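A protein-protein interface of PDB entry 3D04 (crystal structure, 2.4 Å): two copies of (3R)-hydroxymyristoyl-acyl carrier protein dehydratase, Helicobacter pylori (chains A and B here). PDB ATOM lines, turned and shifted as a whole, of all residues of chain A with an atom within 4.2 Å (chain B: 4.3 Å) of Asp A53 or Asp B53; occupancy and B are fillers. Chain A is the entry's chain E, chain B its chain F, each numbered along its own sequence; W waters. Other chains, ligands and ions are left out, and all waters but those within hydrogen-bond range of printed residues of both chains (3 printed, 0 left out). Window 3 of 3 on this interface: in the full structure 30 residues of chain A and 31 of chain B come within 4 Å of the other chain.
Tyr A25 touches Asn B56, and with the chains exchanged Asn A56 touches Tyr B25.
Pro A26 touches Asp B53, and with the chains exchanged Asp A53 touches Pro B26.
Pro A26 touches Val B54, but with the chains exchanged Val A54 does not touch Pro B26 (4.1 Å).
Asp B53 touches its own counterpart, Asp A53.
Positions printed for both chains: 25, 26, 52, 53, 54, 55 and 56.
Of the 6 pairs that touch across the chains among the printed residues, 5 have their exchanged pair printed and touching as well.
Asp A53 touches just these residues of chain B: Pro B26 and Asp B53.
Asp B53 touches two residues of chain A.
Printed residues of chain B within 4 Å of Pro A26: Asp B53 and Val B54.
Of the printed residues of chain A, Pro B26 touches Asp A53 (3.4 Å).
Phe B55 touches none of the printed residues of chain A.
The nearest printed residue of chain A that does not touch Asn B56 is Pro A26 (4.3 Å).
Of the 7 printed residues of chain A, 4 touch a printed residue of chain B.
Of the 7 printed residues of chain B, 5 touch a printed residue of chain A.
Hydrophobic or aromatic side chains of chain B that line the printed part of chain A: Pro B26.
Among the printed residues, 6 pairs touch across the chains.
Among the printed residues, pairs that only touch across the chains: Tyr A25 with Asn B56 (3.4 Å), Pro A26 with Asp B53 (3.3 Å), Pro A26 with Val B54 (3.98 Å), Asp A53 with Pro B26 (3.4 Å), Asp A53 with Asp B53 (3.9 Å) and Asn A56 with Tyr B25 (3.4 Å).
Water W2 lies within hydrogen-bond range of OH of Tyr A25 (2.6 Å), OD2 of Asp B53 (2.6 Å) and OD2 of Asp A53 (3.0 Å).
Water W1 lies within hydrogen-bond range of OD2 of Asp A53, OH of Tyr B25 and OD2 of Asp B53.
Water W3 lies within hydrogen-bond range of the backbone carbonyl oxygen of Tyr B25 (2.6 Å) and the backbone carbonyl oxygen of Asn A56 (3.4 Å).
OD1 of Asp B53 is in hydrogen-bond range of ND2 of Asn B56, 2.8 Å away.
The side-chain carboxylate (OD1) of Asp A53 sits at hydrogen-bond distance from the side-chain amide nitrogen (ND2) of Asn A56 (2.8 Å).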
ATOM      1  N   TYR A  25      17.612   9.856 -32.127  1.00  0.00           N
ATOM      2  CA  TYR A  25      16.364  10.242 -31.467  1.00  0.00           C
ATOM      3  C   TYR A  25      16.167   9.423 -30.183  1.00  0.00           C
ATOM      4  O   TYR A  25      16.345   8.210 -30.218  1.00  0.00           O
ATOM      5  CB  TYR A  25      15.172  10.039 -32.411  1.00  0.00           C
ATOM      6  CG  TYR A  25      13.843  10.417 -31.794  1.00  0.00           C
ATOM      7  CD1 TYR A  25      13.117   9.497 -31.028  1.00  0.00           C
ATOM      8  CD2 TYR A  25      13.316  11.694 -31.962  1.00  0.00           C
ATOM      9  CE1 TYR A  25      11.902   9.838 -30.452  1.00  0.00           C
ATOM     10  CE2 TYR A  25      12.111  12.044 -31.390  1.00  0.00           C
ATOM     11  CZ  TYR A  25      11.408  11.112 -30.634  1.00  0.00           C
ATOM     12  OH  TYR A  25      10.208  11.460 -30.065  1.00  0.00           O
ATOM     13  N   PRO A  26      15.757  10.063 -29.067  1.00  0.00           N
ATOM     14  CA  PRO A  26      15.397  11.471 -28.885  1.00  0.00           C
ATOM     15  C   PRO A  26      16.524  12.349 -28.317  1.00  0.00           C
ATOM     16  O   PRO A  26      16.248  13.264 -27.529  1.00  0.00           O
ATOM     17  CB  PRO A  26      14.264  11.380 -27.865  1.00  0.00           C
ATOM     18  CG  PRO A  26      14.710  10.237 -26.953  1.00  0.00           C
ATOM     19  CD  PRO A  26      15.572   9.310 -27.813  1.00  0.00           C
ATOM     20  N   GLU A  52       7.785  18.198 -29.879  1.00  0.00           N
ATOM     21  CA  GLU A  52       8.863  17.438 -29.271  1.00  0.00           C
ATOM     22  C   GLU A  52       8.338  16.786 -28.002  1.00  0.00           C
ATOM     23  O   GLU A  52       7.594  17.401 -27.248  1.00  0.00           O
ATOM     24  CB  GLU A  52      10.083  18.330 -29.010  1.00  0.00           C
ATOM     25  CG  GLU A  52      10.620  18.995 -30.295  1.00  0.00           C
ATOM     26  CD  GLU A  52      11.922  19.748 -30.105  1.00  0.00           C
ATOM     27  OE1 GLU A  52      12.914  19.129 -29.663  1.00  0.00           O
ATOM     28  OE2 GLU A  52      11.964  20.956 -30.423  1.00  0.00           O
ATOM     29  N   ASP A  53       8.709  15.523 -27.801  1.00  0.00           N
ATOM     30  CA  ASP A  53       8.202  14.715 -26.694  1.00  0.00           C
ATOM     31  C   ASP A  53       8.537  15.291 -25.308  1.00  0.00           C
ATOM     32  O   ASP A  53       7.732  15.170 -24.382  1.00  0.00           O
ATOM     33  CB  ASP A  53       8.691  13.272 -26.836  1.00  0.00           C
ATOM     34  CG  ASP A  53       8.021  12.314 -25.863  1.00  0.00           C
ATOM     35  OD1 ASP A  53       6.856  12.534 -25.466  1.00  0.00           O
ATOM     36  OD2 ASP A  53       8.679  11.317 -25.500  1.00  0.00           O
ATOM     37  N   VAL A  54       9.701  15.938 -25.185  1.00  0.00           N
ATOM     38  CA  VAL A  54      10.132  16.586 -23.932  1.00  0.00           C
ATOM     39  C   VAL A  54       9.068  17.500 -23.348  1.00  0.00           C
ATOM     40  O   VAL A  54       8.960  17.630 -22.128  1.00  0.00           O
ATOM     41  CB  VAL A  54      11.363  17.520 -24.110  1.00  0.00           C
ATOM     42  CG1 VAL A  54      12.389  17.236 -23.034  1.00  0.00           C
ATOM     43  CG2 VAL A  54      11.965  17.398 -25.484  1.00  0.00           C
ATOM     44  N   PHE A  55       8.318  18.155 -24.234  1.00  0.00           N
ATOM     45  CA  PHE A  55       7.354  19.183 -23.842  1.00  0.00           C
ATOM     46  C   PHE A  55       6.121  18.640 -23.110  1.00  0.00           C
ATOM     47  O   PHE A  55       5.445  19.381 -22.390  1.00  0.00           O
ATOM     48  CB  PHE A  55       6.972  20.058 -25.042  1.00  0.00           C
ATOM     49  CG  PHE A  55       8.080  20.983 -25.499  1.00  0.00           C
ATOM     50  CD1 PHE A  55       8.566  20.922 -26.801  1.00  0.00           C
ATOM     51  CD2 PHE A  55       8.640  21.908 -24.621  1.00  0.00           C
ATOM     52  CE1 PHE A  55       9.594  21.779 -27.226  1.00  0.00           C
ATOM     53  CE2 PHE A  55       9.658  22.770 -25.035  1.00  0.00           C
ATOM     54  CZ  PHE A  55      10.138  22.704 -26.340  1.00  0.00           C
ATOM     55  N   ASN A  56       5.853  17.344 -23.274  1.00  0.00           N
ATOM     56  CA  ASN A  56       4.839  16.666 -22.470  1.00  0.00           C
ATOM     57  C   ASN A  56       5.103  16.792 -20.963  1.00  0.00           C
ATOM     58  O   ASN A  56       4.167  16.881 -20.165  1.00  0.00           O
ATOM     59  CB  ASN A  56       4.728  15.194 -22.874  1.00  0.00           C
ATOM     60  CG  ASN A  56       4.008  15.000 -24.200  1.00  0.00           C
ATOM     61  OD1 ASN A  56       2.882  15.467 -24.384  1.00  0.00           O
ATOM     62  ND2 ASN A  56       4.653  14.301 -25.127  1.00  0.00           N
ATOM     63  N   TYR B  25       6.330  13.179 -17.309  1.00  0.00           N
ATOM     64  CA  TYR B  25       6.967  12.325 -18.314  1.00  0.00           C
ATOM     65  C   TYR B  25       7.196  13.068 -19.639  1.00  0.00           C
ATOM     66  O   TYR B  25       6.281  13.720 -20.133  1.00  0.00           O
ATOM     67  CB  TYR B  25       6.126  11.058 -18.558  1.00  0.00           C
ATOM     68  CG  TYR B  25       6.752  10.133 -19.577  1.00  0.00           C
ATOM     69  CD1 TYR B  25       6.527  10.314 -20.940  1.00  0.00           C
ATOM     70  CD2 TYR B  25       7.598   9.104 -19.179  1.00  0.00           C
ATOM     71  CE1 TYR B  25       7.123   9.492 -21.879  1.00  0.00           C
ATOM     72  CE2 TYR B  25       8.198   8.273 -20.112  1.00  0.00           C
ATOM     73  CZ  TYR B  25       7.956   8.473 -21.460  1.00  0.00           C
ATOM     74  OH  TYR B  25       8.552   7.654 -22.388  1.00  0.00           O
ATOM     75  N   PRO B  26       8.394  12.933 -20.249  1.00  0.00           N
ATOM     76  CA  PRO B  26       9.565  12.156 -19.846  1.00  0.00           C
ATOM     77  C   PRO B  26      10.662  12.977 -19.165  1.00  0.00           C
ATOM     78  O   PRO B  26      11.848  12.707 -19.369  1.00  0.00           O
ATOM     79  CB  PRO B  26      10.081  11.629 -21.183  1.00  0.00           C
ATOM     80  CG  PRO B  26       9.731  12.741 -22.170  1.00  0.00           C
ATOM     81  CD  PRO B  26       8.619  13.577 -21.557  1.00  0.00           C
ATOM     82  N   GLU B  52      13.568   2.901 -21.075  1.00  0.00           N
ATOM     83  CA  GLU B  52      13.410   4.359 -21.113  1.00  0.00           C
ATOM     84  C   GLU B  52      13.735   4.838 -22.523  1.00  0.00           C
ATOM     85  O   GLU B  52      14.656   4.324 -23.151  1.00  0.00           O
ATOM     86  CB  GLU B  52      14.296   5.056 -20.066  1.00  0.00           C
ATOM     87  CG  GLU B  52      14.070   4.563 -18.628  1.00  0.00           C
ATOM     88  CD  GLU B  52      14.919   5.283 -17.591  1.00  0.00           C
ATOM     89  OE1 GLU B  52      14.792   6.518 -17.468  1.00  0.00           O
ATOM     90  OE2 GLU B  52      15.695   4.615 -16.870  1.00  0.00           O
ATOM     91  N   ASP B  53      12.960   5.805 -23.017  1.00  0.00           N
ATOM     92  CA  ASP B  53      13.055   6.270 -24.403  1.00  0.00           C
ATOM     93  C   ASP B  53      14.411   6.883 -24.741  1.00  0.00           C
ATOM     94  O   ASP B  53      14.885   6.729 -25.869  1.00  0.00           O
ATOM     95  CB  ASP B  53      11.923   7.261 -24.714  1.00  0.00           C
ATOM     96  CG  ASP B  53      11.638   7.401 -26.209  1.00  0.00           C
ATOM     97  OD1 ASP B  53      12.180   6.647 -27.044  1.00  0.00           O
ATOM     98  OD2 ASP B  53      10.848   8.279 -26.562  1.00  0.00           O
ATOM     99  N   VAL B  54      15.033   7.564 -23.774  1.00  0.00           N
ATOM    100  CA  VAL B  54      16.364   8.163 -23.984  1.00  0.00           C
ATOM    101  C   VAL B  54      17.397   7.199 -24.565  1.00  0.00           C
ATOM    102  O   VAL B  54      18.240   7.614 -25.363  1.00  0.00           O
ATOM    103  CB  VAL B  54      17.020   8.760 -22.694  1.00  0.00           C
ATOM    104  CG1 VAL B  54      16.876  10.265 -22.659  1.00  0.00           C
ATOM    105  CG2 VAL B  54      16.542   8.063 -21.413  1.00  0.00           C
ATOM    106  N   PHE B  55      17.348   5.937 -24.140  1.00  0.00           N
ATOM    107  CA  PHE B  55      18.367   4.957 -24.531  1.00  0.00           C
ATOM    108  C   PHE B  55      18.322   4.583 -26.008  1.00  0.00           C
ATOM    109  O   PHE B  55      19.281   4.017 -26.526  1.00  0.00           O
ATOM    110  CB  PHE B  55      18.341   3.720 -23.624  1.00  0.00           C
ATOM    111  CG  PHE B  55      18.775   4.007 -22.216  1.00  0.00           C
ATOM    112  CD1 PHE B  55      17.903   3.814 -21.149  1.00  0.00           C
ATOM    113  CD2 PHE B  55      20.049   4.520 -21.959  1.00  0.00           C
ATOM    114  CE1 PHE B  55      18.301   4.105 -19.840  1.00  0.00           C
ATOM    115  CE2 PHE B  55      20.455   4.807 -20.656  1.00  0.00           C
ATOM    116  CZ  PHE B  55      19.576   4.607 -19.597  1.00  0.00           C
ATOM    117  N   ASN B  56      17.222   4.918 -26.683  1.00  0.00           N
ATOM    118  CA  ASN B  56      17.142   4.786 -28.139  1.00  0.00           C
ATOM    119  C   ASN B  56      18.180   5.655 -28.848  1.00  0.00           C
ATOM    120  O   ASN B  56      18.718   5.265 -29.883  1.00  0.00           O
ATOM    121  CB  ASN B  56      15.735   5.108 -28.653  1.00  0.00           C
ATOM    122  CG  ASN B  56      14.734   3.987 -28.382  1.00  0.00           C
ATOM    123  OD1 ASN B  56      14.960   2.828 -28.744  1.00  0.00           O
ATOM    124  ND2 ASN B  56      13.611   4.337 -27.766  1.00  0.00           N
HETATM  125  O   HOH W   1       8.565   8.780 -24.840  1.00  0.00           O
HETATM  126  O   HOH W   2       9.589   9.976 -28.057  1.00  0.00           O
HETATM  127  O   HOH W   3       3.731  13.575 -19.511  1.00  0.00           O
